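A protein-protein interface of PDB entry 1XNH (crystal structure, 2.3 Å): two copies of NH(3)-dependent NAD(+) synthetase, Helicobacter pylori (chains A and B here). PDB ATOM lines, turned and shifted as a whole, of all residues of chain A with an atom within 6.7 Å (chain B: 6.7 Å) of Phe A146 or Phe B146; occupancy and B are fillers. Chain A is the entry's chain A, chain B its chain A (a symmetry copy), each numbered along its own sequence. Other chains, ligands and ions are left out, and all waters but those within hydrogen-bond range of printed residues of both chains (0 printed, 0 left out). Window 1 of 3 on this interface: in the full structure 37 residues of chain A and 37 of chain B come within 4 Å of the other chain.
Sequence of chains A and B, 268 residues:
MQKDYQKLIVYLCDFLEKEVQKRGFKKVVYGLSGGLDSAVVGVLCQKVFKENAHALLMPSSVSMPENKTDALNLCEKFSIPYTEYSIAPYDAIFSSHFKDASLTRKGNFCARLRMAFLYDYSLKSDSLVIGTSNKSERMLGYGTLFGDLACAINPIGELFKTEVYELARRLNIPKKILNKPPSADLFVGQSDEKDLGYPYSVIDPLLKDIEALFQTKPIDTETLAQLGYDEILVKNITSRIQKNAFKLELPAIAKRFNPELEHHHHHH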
ATOM      1  N   ASN A 108      13.304  23.727 -17.551  1.00  0.00           N
ATOM      2  CA  ASN A 108      13.064  22.683 -18.529  1.00  0.00           C
ATOM      3  C   ASN A 108      13.574  23.115 -19.914  1.00  0.00           C
ATOM      4  O   ASN A 108      14.277  22.351 -20.619  1.00  0.00           O
ATOM      5  CB  ASN A 108      11.581  22.343 -18.558  1.00  0.00           C
ATOM      6  CG  ASN A 108      11.139  21.684 -17.259  1.00  0.00           C
ATOM      7  OD1 ASN A 108      11.988  21.326 -16.445  1.00  0.00           O
ATOM      8  ND2 ASN A 108       9.836  21.500 -17.066  1.00  0.00           N
ATOM      9  N   ALA A 111      17.448  23.053 -20.245  1.00  0.00           N
ATOM     10  CA  ALA A 111      17.952  21.661 -20.282  1.00  0.00           C
ATOM     11  C   ALA A 111      17.683  21.004 -21.681  1.00  0.00           C
ATOM     12  O   ALA A 111      18.409  20.100 -22.096  1.00  0.00           O
ATOM     13  CB  ALA A 111      17.295  20.855 -19.158  1.00  0.00           C
ATOM     14  N   ARG A 112      16.646  21.478 -22.378  1.00  0.00           N
ATOM     15  CA  ARG A 112      16.321  21.006 -23.700  1.00  0.00           C
ATOM     16  C   ARG A 112      17.236  21.650 -24.757  1.00  0.00           C
ATOM     17  O   ARG A 112      17.447  21.070 -25.857  1.00  0.00           O
ATOM     18  CB  ARG A 112      14.875  21.295 -24.033  1.00  0.00           C
ATOM     19  CG  ARG A 112      13.996  20.132 -23.628  1.00  0.00           C
ATOM     20  CD  ARG A 112      12.553  20.508 -23.427  1.00  0.00           C
ATOM     21  NE  ARG A 112      11.887  19.399 -22.766  1.00  0.00           N
ATOM     22  CZ  ARG A 112      10.983  19.531 -21.802  1.00  0.00           C
ATOM     23  NH1 ARG A 112      10.618  20.738 -21.385  1.00  0.00           N
ATOM     24  NH2 ARG A 112      10.442  18.451 -21.253  1.00  0.00           N
ATOM     25  N   LEU A 113      17.757  22.844 -24.437  1.00  0.00           N
ATOM     26  CA  LEU A 113      18.707  23.579 -25.286  1.00  0.00           C
ATOM     27  C   LEU A 113      20.046  22.839 -25.261  1.00  0.00           C
ATOM     28  O   LEU A 113      20.620  22.581 -26.303  1.00  0.00           O
ATOM     29  CB  LEU A 113      18.922  25.025 -24.765  1.00  0.00           C
ATOM     30  CG  LEU A 113      17.706  25.921 -24.993  1.00  0.00           C
ATOM     31  CD1 LEU A 113      17.709  26.987 -23.915  1.00  0.00           C
ATOM     32  CD2 LEU A 113      17.686  26.505 -26.426  1.00  0.00           C
ATOM     33  N   MET A 115      20.527  19.901 -24.722  1.00  0.00           N
ATOM     34  CA  MET A 115      20.317  18.636 -25.392  1.00  0.00           C
ATOM     35  C   MET A 115      20.447  18.837 -26.921  1.00  0.00           C
ATOM     36  O   MET A 115      21.027  17.997 -27.625  1.00  0.00           O
ATOM     37  CB  MET A 115      18.933  18.108 -25.037  1.00  0.00           C
ATOM     38  CG  MET A 115      18.487  16.873 -25.772  1.00  0.00           C
ATOM     39  SD  MET A 115      17.962  17.127 -27.519  1.00  0.00           S
ATOM     40  CE  MET A 115      16.286  17.880 -27.330  1.00  0.00           C
ATOM     41  N   ALA A 116      19.911  19.951 -27.418  1.00  0.00           N
ATOM     42  CA  ALA A 116      19.964  20.271 -28.829  1.00  0.00           C
ATOM     43  C   ALA A 116      21.406  20.423 -29.305  1.00  0.00           C
ATOM     44  O   ALA A 116      21.775  19.963 -30.378  1.00  0.00           O
ATOM     45  CB  ALA A 116      19.181  21.553 -29.109  1.00  0.00           C
ATOM     46  N   TYR A 119      23.400  17.082 -29.258  1.00  0.00           N
ATOM     47  CA  TYR A 119      23.112  16.286 -30.443  1.00  0.00           C
ATOM     48  C   TYR A 119      23.545  16.945 -31.764  1.00  0.00           C
ATOM     49  O   TYR A 119      23.829  16.235 -32.732  1.00  0.00           O
ATOM     50  CB  TYR A 119      21.635  15.889 -30.525  1.00  0.00           C
ATOM     51  CG  TYR A 119      21.378  14.558 -29.850  1.00  0.00           C
ATOM     52  CD1 TYR A 119      21.123  14.484 -28.483  1.00  0.00           C
ATOM     53  CD2 TYR A 119      21.435  13.359 -30.580  1.00  0.00           C
ATOM     54  CE1 TYR A 119      20.931  13.262 -27.862  1.00  0.00           C
ATOM     55  CE2 TYR A 119      21.241  12.135 -29.965  1.00  0.00           C
ATOM     56  CZ  TYR A 119      20.986  12.098 -28.595  1.00  0.00           C
ATOM     57  OH  TYR A 119      20.769  10.885 -27.968  1.00  0.00           O
ATOM     58  N   VAL A 129      26.041  10.793 -27.784  1.00  0.00           N
ATOM     59  CA  VAL A 129      25.734  11.488 -26.542  1.00  0.00           C
ATOM     60  C   VAL A 129      25.650  10.474 -25.390  1.00  0.00           C
ATOM     61  O   VAL A 129      25.060   9.423 -25.529  1.00  0.00           O
ATOM     62  CB  VAL A 129      24.382  12.252 -26.658  1.00  0.00           C
ATOM     63  CG1 VAL A 129      24.092  13.098 -25.377  1.00  0.00           C
ATOM     64  CG2 VAL A 129      24.398  13.112 -27.891  1.00  0.00           C
ATOM     65  N   THR A 144      14.683  16.244 -16.571  1.00  0.00           N
ATOM     66  CA  THR A 144      13.941  16.762 -17.706  1.00  0.00           C
ATOM     67  C   THR A 144      13.887  15.782 -18.873  1.00  0.00           C
ATOM     68  O   THR A 144      14.927  15.387 -19.429  1.00  0.00           O
ATOM     69  CB  THR A 144      14.540  18.088 -18.190  1.00  0.00           C
ATOM     70  OG1 THR A 144      14.650  19.001 -17.088  1.00  0.00           O
ATOM     71  CG2 THR A 144      13.649  18.694 -19.226  1.00  0.00           C
ATOM     72  N   LEU A 145      12.669  15.401 -19.242  1.00  0.00           N
ATOM     73  CA  LEU A 145      12.447  14.476 -20.342  1.00  0.00           C
ATOM     74  C   LEU A 145      12.878  15.178 -21.615  1.00  0.00           C
ATOM     75  O   LEU A 145      12.562  16.353 -21.834  1.00  0.00           O
ATOM     76  CB  LEU A 145      10.970  14.105 -20.422  1.00  0.00           C
ATOM     77  CG  LEU A 145      10.485  13.164 -21.537  1.00  0.00           C
ATOM     78  CD1 LEU A 145      11.039  11.745 -21.359  1.00  0.00           C
ATOM     79  CD2 LEU A 145       8.953  13.193 -21.506  1.00  0.00           C
ATOM     80  N   PHE A 146      13.617  14.457 -22.448  1.00  0.00           N
ATOM     81  CA  PHE A 146      14.132  14.991 -23.697  1.00  0.00           C
ATOM     82  C   PHE A 146      15.039  16.182 -23.417  1.00  0.00           C
ATOM     83  O   PHE A 146      15.275  17.035 -24.287  1.00  0.00           O
ATOM     84  CB  PHE A 146      12.985  15.375 -24.612  1.00  0.00           C
ATOM     85  CG  PHE A 146      11.954  14.288 -24.779  1.00  0.00           C
ATOM     86  CD1 PHE A 146      10.592  14.591 -24.728  1.00  0.00           C
ATOM     87  CD2 PHE A 146      12.334  12.972 -24.987  1.00  0.00           C
ATOM     88  CE1 PHE A 146       9.634  13.603 -24.894  1.00  0.00           C
ATOM     89  CE2 PHE A 146      11.379  11.969 -25.153  1.00  0.00           C
ATOM     90  CZ  PHE A 146      10.029  12.292 -25.100  1.00  0.00           C
ATOM     91  N   GLY A 147      15.548  16.221 -22.180  1.00  0.00           N
ATOM     92  CA  GLY A 147      16.472  17.265 -21.738  1.00  0.00           C
ATOM     93  C   GLY A 147      17.789  16.634 -21.295  1.00  0.00           C
ATOM     94  O   GLY A 147      18.615  16.234 -22.111  1.00  0.00           O
ATOM     95  N   ASP A 148      17.980  16.534 -19.988  1.00  0.00           N
ATOM     96  CA  ASP A 148      19.187  15.950 -19.441  1.00  0.00           C
ATOM     97  C   ASP A 148      19.090  14.431 -19.371  1.00  0.00           C
ATOM     98  O   ASP A 148      20.054  13.766 -19.006  1.00  0.00           O
ATOM     99  CB  ASP A 148      19.459  16.548 -18.055  1.00  0.00           C
ATOM    100  CG  ASP A 148      18.286  16.374 -17.095  1.00  0.00           C
ATOM    101  OD1 ASP A 148      17.142  16.789 -17.424  1.00  0.00           O
ATOM    102  OD2 ASP A 148      18.499  15.826 -15.997  1.00  0.00           O
ATOM    103  N   LEU A 149      17.921  13.887 -19.711  1.00  0.00           N
ATOM    104  CA  LEU A 149      17.698  12.430 -19.727  1.00  0.00           C
ATOM    105  C   LEU A 149      17.776  11.887 -21.146  1.00  0.00           C
ATOM    106  O   LEU A 149      17.727  10.683 -21.364  1.00  0.00           O
ATOM    107  CB  LEU A 149      16.323  12.080 -19.152  1.00  0.00           C
ATOM    108  CG  LEU A 149      16.085  12.352 -17.660  1.00  0.00           C
ATOM    109  CD1 LEU A 149      14.600  12.577 -17.443  1.00  0.00           C
ATOM    110  CD2 LEU A 149      16.598  11.165 -16.844  1.00  0.00           C
ATOM    111  N   ALA A 150      17.886  12.796 -22.108  1.00  0.00           N
ATOM    112  CA  ALA A 150      17.994  12.438 -23.523  1.00  0.00           C
ATOM    113  C   ALA A 150      19.460  12.101 -23.870  1.00  0.00           C
ATOM    114  O   ALA A 150      20.303  12.988 -23.934  1.00  0.00           O
ATOM    115  CB  ALA A 150      17.508  13.593 -24.380  1.00  0.00           C
ATOM    116  N   CYS A 151      19.760  10.824 -24.075  1.00  0.00           N
ATOM    117  CA  CYS A 151      21.117  10.385 -24.396  1.00  0.00           C
ATOM    118  C   CYS A 151      20.995   9.053 -25.071  1.00  0.00           C
ATOM    119  O   CYS A 151      19.927   8.436 -25.035  1.00  0.00           O
ATOM    120  CB  CYS A 151      21.941  10.159 -23.140  1.00  0.00           C
ATOM    121  SG  CYS A 151      21.329   8.733 -22.176  1.00  0.00           S
ATOM    122  N   ALA A 152      22.098   8.576 -25.635  1.00  0.00           N
ATOM    123  CA  ALA A 152      22.083   7.294 -26.321  1.00  0.00           C
ATOM    124  C   ALA A 152      22.492   6.215 -25.328  1.00  0.00           C
ATOM    125  O   ALA A 152      21.933   5.123 -25.323  1.00  0.00           O
ATOM    126  CB  ALA A 152      23.050   7.325 -27.525  1.00  0.00           C
ATOM    127  N   LYS A 247       8.525   8.851 -17.600  1.00  0.00           N
ATOM    128  CA  LYS A 247       9.721   9.432 -18.176  1.00  0.00           C
ATOM    129  C   LYS A 247      10.734   8.405 -18.689  1.00  0.00           C
ATOM    130  O   LYS A 247      11.458   8.664 -19.657  1.00  0.00           O
ATOM    131  CB  LYS A 247      10.392  10.354 -17.160  1.00  0.00           C
ATOM    132  CG  LYS A 247       9.563  11.584 -16.823  1.00  0.00           C
ATOM    133  CD  LYS A 247      10.330  12.523 -15.907  1.00  0.00           C
ATOM    134  CE  LYS A 247       9.486  13.723 -15.503  1.00  0.00           C
ATOM    135  NZ  LYS A 247      10.280  14.790 -14.825  1.00  0.00           N
ATOM    136  N   PRO A 251       7.298   6.093 -25.565  1.00  0.00           N
ATOM    137  CA  PRO A 251       5.992   6.724 -25.795  1.00  0.00           C
ATOM    138  C   PRO A 251       4.914   5.700 -26.096  1.00  0.00           C
ATOM    139  O   PRO A 251       5.200   4.621 -26.607  1.00  0.00           O
ATOM    140  CB  PRO A 251       6.256   7.629 -26.994  1.00  0.00           C
ATOM    141  CG  PRO A 251       7.347   6.899 -27.733  1.00  0.00           C
ATOM    142  CD  PRO A 251       8.259   6.478 -26.618  1.00  0.00           C
ATOM    143  N   ASN B 108      17.562  19.809 -37.553  1.00  0.00           N
ATOM    144  CA  ASN B 108      17.469  19.085 -36.299  1.00  0.00           C
ATOM    145  C   ASN B 108      17.223  20.058 -35.133  1.00  0.00           C
ATOM    146  O   ASN B 108      16.335  19.837 -34.274  1.00  0.00           O
ATOM    147  CB  ASN B 108      18.733  18.265 -36.089  1.00  0.00           C
ATOM    148  CG  ASN B 108      18.840  17.141 -37.111  1.00  0.00           C
ATOM    149  OD1 ASN B 108      17.874  16.887 -37.830  1.00  0.00           O
ATOM    150  ND2 ASN B 108      19.979  16.458 -37.169  1.00  0.00           N
ATOM    151  N   ALA B 111      13.605  21.477 -35.013  1.00  0.00           N
ATOM    152  CA  ALA B 111      12.642  20.432 -34.597  1.00  0.00           C
ATOM    153  C   ALA B 111      12.737  20.165 -33.054  1.00  0.00           C
ATOM    154  O   ALA B 111      11.761  19.743 -32.432  1.00  0.00           O
ATOM    155  CB  ALA B 111      12.906  19.153 -35.396  1.00  0.00           C
ATOM    156  N   ARG B 112      13.911  20.422 -32.471  1.00  0.00           N
ATOM    157  CA  ARG B 112      14.120  20.276 -31.052  1.00  0.00           C
ATOM    158  C   ARG B 112      13.554  21.483 -30.283  1.00  0.00           C
ATOM    159  O   ARG B 112      13.212  21.367 -29.075  1.00  0.00           O
ATOM    160  CB  ARG B 112      15.590  20.116 -30.740  1.00  0.00           C
ATOM    161  CG  ARG B 112      15.975  18.652 -30.736  1.00  0.00           C
ATOM    162  CD  ARG B 112      17.444  18.414 -30.958  1.00  0.00           C
ATOM    163  NE  ARG B 112      17.634  16.999 -31.226  1.00  0.00           N
ATOM    164  CZ  ARG B 112      18.471  16.511 -32.134  1.00  0.00           C
ATOM    165  NH1 ARG B 112      19.217  17.329 -32.867  1.00  0.00           N
ATOM    166  NH2 ARG B 112      18.561  15.199 -32.311  1.00  0.00           N
ATOM    167  N   LEU B 113      13.475  22.634 -30.969  1.00  0.00           N
ATOM    168  CA  LEU B 113      12.897  23.873 -30.427  1.00  0.00           C
ATOM    169  C   LEU B 113      11.383  23.685 -30.308  1.00  0.00           C
ATOM    170  O   LEU B 113      10.814  23.966 -29.270  1.00  0.00           O
ATOM    171  CB  LEU B 113      13.182  25.079 -31.361  1.00  0.00           C
ATOM    172  CG  LEU B 113      14.647  25.509 -31.340  1.00  0.00           C
ATOM    173  CD1 LEU B 113      14.964  26.139 -32.682  1.00  0.00           C
ATOM    174  CD2 LEU B 113      14.953  26.441 -30.143  1.00  0.00           C
ATOM    175  N   MET B 115       9.859  21.092 -29.986  1.00  0.00           N
ATOM    176  CA  MET B 115       9.643  20.091 -28.963  1.00  0.00           C
ATOM    177  C   MET B 115       9.678  20.765 -27.569  1.00  0.00           C
ATOM    178  O   MET B 115       8.877  20.433 -26.684  1.00  0.00           O
ATOM    179  CB  MET B 115      10.727  19.026 -29.069  1.00  0.00           C
ATOM    180  CG  MET B 115      10.744  17.988 -27.980  1.00  0.00           C
ATOM    181  SD  MET B 115      11.421  18.540 -26.359  1.00  0.00           S
ATOM    182  CE  MET B 115      13.242  18.557 -26.668  1.00  0.00           C
ATOM    183  N   ALA B 116      10.601  21.709 -27.394  1.00  0.00           N
ATOM    184  CA  ALA B 116      10.744  22.427 -26.144  1.00  0.00           C
ATOM    185  C   ALA B 116       9.479  23.214 -25.814  1.00  0.00           C
ATOM    186  O   ALA B 116       9.031  23.252 -24.675  1.00  0.00           O
ATOM    187  CB  ALA B 116      11.946  23.368 -26.210  1.00  0.00           C
ATOM    188  N   TYR B 119       6.428  20.944 -24.988  1.00  0.00           N
ATOM    189  CA  TYR B 119       6.479  20.485 -23.607  1.00  0.00           C
ATOM    190  C   TYR B 119       6.382  21.611 -22.564  1.00  0.00           C
ATOM    191  O   TYR B 119       5.919  21.367 -21.447  1.00  0.00           O
ATOM    192  CB  TYR B 119       7.720  19.631 -23.330  1.00  0.00           C
ATOM    193  CG  TYR B 119       7.449  18.160 -23.569  1.00  0.00           C
ATOM    194  CD1 TYR B 119       7.586  17.603 -24.837  1.00  0.00           C
ATOM    195  CD2 TYR B 119       7.010  17.331 -22.523  1.00  0.00           C
ATOM    196  CE1 TYR B 119       7.296  16.268 -25.061  1.00  0.00           C
ATOM    197  CE2 TYR B 119       6.722  15.996 -22.740  1.00  0.00           C
ATOM    198  CZ  TYR B 119       6.871  15.470 -24.022  1.00  0.00           C
ATOM    199  OH  TYR B 119       6.608  14.132 -24.251  1.00  0.00           O
ATOM    200  N   VAL B 129       1.646  15.871 -24.692  1.00  0.00           N
ATOM    201  CA  VAL B 129       2.111  16.014 -26.064  1.00  0.00           C
ATOM    202  C   VAL B 129       1.765  14.745 -26.861  1.00  0.00           C
ATOM    203  O   VAL B 129       1.948  13.644 -26.387  1.00  0.00           O
ATOM    204  CB  VAL B 129       3.650  16.245 -26.103  1.00  0.00           C
ATOM    205  CG1 VAL B 129       4.150  16.516 -27.559  1.00  0.00           C
ATOM    206  CG2 VAL B 129       4.009  17.376 -25.180  1.00  0.00           C
ATOM    207  N   THR B 144      13.560  13.373 -36.365  1.00  0.00           N
ATOM    208  CA  THR B 144      14.500  13.902 -35.393  1.00  0.00           C
ATOM    209  C   THR B 144      14.266  13.357 -33.988  1.00  0.00           C
ATOM    210  O   THR B 144      13.186  13.539 -33.399  1.00  0.00           O
ATOM    211  CB  THR B 144      14.439  15.434 -35.354  1.00  0.00           C
ATOM    212  OG1 THR B 144      14.600  15.959 -36.680  1.00  0.00           O
ATOM    213  CG2 THR B 144      15.543  15.959 -34.494  1.00  0.00           C
ATOM    214  N   LEU B 145      15.288  12.694 -33.457  1.00  0.00           N
ATOM    215  CA  LEU B 145      15.226  12.117 -32.123  1.00  0.00           C
ATOM    216  C   LEU B 145      15.145  13.268 -31.138  1.00  0.00           C
ATOM    217  O   LEU B 145      15.869  14.262 -31.258  1.00  0.00           O
ATOM    218  CB  LEU B 145      16.478  11.287 -31.856  1.00  0.00           C
ATOM    219  CG  LEU B 145      16.656  10.607 -30.488  1.00  0.00           C
ATOM    220  CD1 LEU B 145      15.625   9.493 -30.272  1.00  0.00           C
ATOM    221  CD2 LEU B 145      18.094  10.079 -30.442  1.00  0.00           C
ATOM    222  N   PHE B 146      14.245  13.136 -30.173  1.00  0.00           N
ATOM    223  CA  PHE B 146      14.024  14.160 -29.167  1.00  0.00           C
ATOM    224  C   PHE B 146      13.585  15.456 -29.834  1.00  0.00           C
ATOM    225  O   PHE B 146      13.717  16.553 -29.267  1.00  0.00           O
ATOM    226  CB  PHE B 146      15.281  14.361 -28.342  1.00  0.00           C
ATOM    227  CG  PHE B 146      15.865  13.080 -27.807  1.00  0.00           C
ATOM    228  CD1 PHE B 146      17.241  12.849 -27.869  1.00  0.00           C
ATOM    229  CD2 PHE B 146      15.054  12.108 -27.242  1.00  0.00           C
ATOM    230  CE1 PHE B 146      17.792  11.680 -27.367  1.00  0.00           C
ATOM    231  CE2 PHE B 146      15.598  10.927 -26.736  1.00  0.00           C
ATOM    232  CZ  PHE B 146      16.969  10.718 -26.807  1.00  0.00           C
ATOM    233  N   GLY B 147      13.056  15.308 -31.054  1.00  0.00           N
ATOM    234  CA  GLY B 147      12.540  16.434 -31.834  1.00  0.00           C
ATOM    235  C   GLY B 147      11.063  16.212 -32.144  1.00  0.00           C
ATOM    236  O   GLY B 147      10.195  16.391 -31.293  1.00  0.00           O
ATOM    237  N   ASP B 148      10.776  15.807 -33.372  1.00  0.00           N
ATOM    238  CA  ASP B 148       9.413  15.558 -33.790  1.00  0.00           C
ATOM    239  C   ASP B 148       8.959  14.155 -33.404  1.00  0.00           C
ATOM    240  O   ASP B 148       7.802  13.800 -33.610  1.00  0.00           O
ATOM    241  CB  ASP B 148       9.295  15.778 -35.303  1.00  0.00           C
ATOM    242  CG  ASP B 148      10.274  14.924 -36.103  1.00  0.00           C
ATOM    243  OD1 ASP B 148      11.507  14.982 -35.847  1.00  0.00           O
ATOM    244  OD2 ASP B 148       9.820  14.190 -37.001  1.00  0.00           O
ATOM    245  N   LEU B 149       9.875  13.356 -32.855  1.00  0.00           N
ATOM    246  CA  LEU B 149       9.566  11.989 -32.400  1.00  0.00           C
ATOM    247  C   LEU B 149       9.379  11.952 -30.890  1.00  0.00           C
ATOM    248  O   LEU B 149       9.008  10.930 -30.326  1.00  0.00           O
ATOM    249  CB  LEU B 149      10.692  11.021 -32.769  1.00  0.00           C
ATOM    250  CG  LEU B 149      10.928  10.738 -34.259  1.00  0.00           C
ATOM    251  CD1 LEU B 149      12.382  10.346 -34.450  1.00  0.00           C
ATOM    252  CD2 LEU B 149       9.982   9.628 -34.717  1.00  0.00           C
ATOM    253  N   ALA B 150       9.652  13.080 -30.245  1.00  0.00           N
ATOM    254  CA  ALA B 150       9.503  13.217 -28.796  1.00  0.00           C
ATOM    255  C   ALA B 150       8.034  13.541 -28.447  1.00  0.00           C
ATOM    256  O   ALA B 150       7.567  14.646 -28.693  1.00  0.00           O
ATOM    257  CB  ALA B 150      10.414  14.321 -28.291  1.00  0.00           C
ATOM    258  N   CYS B 151       7.312  12.575 -27.892  1.00  0.00           N
ATOM    259  CA  CYS B 151       5.907  12.763 -27.533  1.00  0.00           C
ATOM    260  C   CYS B 151       5.585  11.735 -26.490  1.00  0.00           C
ATOM    261  O   CYS B 151       6.360  10.798 -26.284  1.00  0.00           O
ATOM    262  CB  CYS B 151       4.988  12.486 -28.710  1.00  0.00           C
ATOM    263  SG  CYS B 151       4.999  10.720 -29.177  1.00  0.00           S
ATOM    264  N   ALA B 152       4.417  11.871 -25.873  1.00  0.00           N
ATOM    265  CA  ALA B 152       4.013  10.929 -24.840  1.00  0.00           C
ATOM    266  C   ALA B 152       3.193   9.826 -25.494  1.00  0.00           C
ATOM    267  O   ALA B 152       3.326   8.657 -25.147  1.00  0.00           O
ATOM    268  CB  ALA B 152       3.189  11.654 -23.754  1.00  0.00           C
ATOM    269  N   LYS B 247      16.733   4.927 -32.869  1.00  0.00           N
ATOM    270  CA  LYS B 247      15.856   6.036 -32.557  1.00  0.00           C
ATOM    271  C   LYS B 247      14.574   5.637 -31.821  1.00  0.00           C
ATOM    272  O   LYS B 247      14.044   6.408 -31.014  1.00  0.00           O
ATOM    273  CB  LYS B 247      15.502   6.795 -33.834  1.00  0.00           C
ATOM    274  CG  LYS B 247      16.694   7.492 -34.471  1.00  0.00           C
ATOM    275  CD  LYS B 247      16.261   8.329 -35.663  1.00  0.00           C
ATOM    276  CE  LYS B 247      17.453   8.974 -36.355  1.00  0.00           C
ATOM    277  NZ  LYS B 247      17.055  10.004 -37.360  1.00  0.00           N
ATOM    278  N   PRO B 251      17.338   4.384 -24.390  1.00  0.00           N
ATOM    279  CA  PRO B 251      18.794   4.548 -24.284  1.00  0.00           C
ATOM    280  C   PRO B 251      19.452   3.344 -23.636  1.00  0.00           C
ATOM    281  O   PRO B 251      18.830   2.639 -22.847  1.00  0.00           O
ATOM    282  CB  PRO B 251      18.936   5.796 -23.420  1.00  0.00           C
ATOM    283  CG  PRO B 251      17.700   5.754 -22.561  1.00  0.00           C
ATOM    284  CD  PRO B 251      16.637   5.377 -23.552  1.00  0.00           C
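Tyr A119 touches Leu B145, and with the chains exchanged Leu A145 touches Tyr B119.
Tyr A119 touches Phe B146, and with the chains exchanged Phe A146 touches Tyr B119.
Phe A146 touches its own counterpart, Phe B146.
Phe A146 touches Cys B151, and with the chains exchanged Cys A151 touches Phe B146.
Of the 22 pairs that touch across the chains among the printed residues, 22 have their exchanged pair printed and touching as well.
The guanidinium group (NH2) of Arg A112 lies within hydrogen-bond range of the backbone carbonyl oxygen (O) of Leu A145, 3.0 Å away.
The backbone carbonyl oxygen (O) of Val A129 lies within hydrogen-bond range of the backbone NH (N) of Ala A152.
NH2 of Arg B112 sits at hydrogen-bond distance from O of Leu B145, 3.0 Å away.
O of Val B129 is in hydrogen-bond range of N of Ala B152, 3.1 Å away.
Hydrophobic or aromatic side chains of chain B within 4 Å of the printed part of chain A: Met B115, Tyr B119, Leu B145, Phe B146, Ala B150 and Pro B251.
Along chain B the printed residues that touch a printed residue of chain A span positions 112 to 251.
Printed residues of chain A that touch a printed residue of chain B: Arg A112, Met A115, Ala A116, Tyr A119, Leu A145, Phe A146, Ala A150, Cys A151, Ala A152 and Pro A251.
Hydrophobic or aromatic side chains of chain A that line the printed part of chain B: Met A115, Tyr A119, Leu A145, Phe A146, Ala A150 and Pro A251.
Along chain A the printed residues that touch a printed residue of chain B span positions 112 to 251.
Among the printed residues, 22 pairs touch across the chains.
The side-chain sulfur (SD) of Met B115 lies close to the guanidinium group (NE) of Arg A112, at 3.7 Å.
NE of Arg B112 sits close to SD of Met A115, at 3.7 Å.
Met B115 touches Met A115.
CD of Arg B112 touches CA of Ala A116 (3.8 Å).
Leu B145 touches Tyr A119.
Tyr B119 touches Leu A145 (OH to CD2, 3.7 Å).
CE of Met B115 touches O of Phe A146 (3.5 Å).
Phe A146 touches Ala B150 (CE1 to CB, 3.6 Å).
Ala A150 touches Phe B146.
Cys A151 touches Pro B251.
Ala A152 touches Pro B251.
Cys B151 touches Pro A251 (O to CB, 3.2 Å).
Val A129 touches none of the printed residues of chain B.
Phe A146 touches five residues of chain B.
Of the printed residues of chain B, Ala A152 touches Pro B251 (3.4 Å).
Of the printed residues of chain A, Arg B112 touches Met A115 (3.5 Å), Ala A116 (3.8 Å) and Tyr A119 (3.6 Å).
Of the printed residues of chain A, Tyr B119 touches Arg A112, Leu A145 and Phe A146.
Thr B144 touches none of the printed residues of chain A.
Phe B146 touches five residues of chain A.
Printed residues of chain A within 4 Å of Ala B150: Phe A146.
The nearest residue of chain B that does not touch Phe A146 is Leu B149 (5.5 Å).
The nearest printed residue of chain A that does not touch Met B115 is Leu A145 (5.2 Å).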
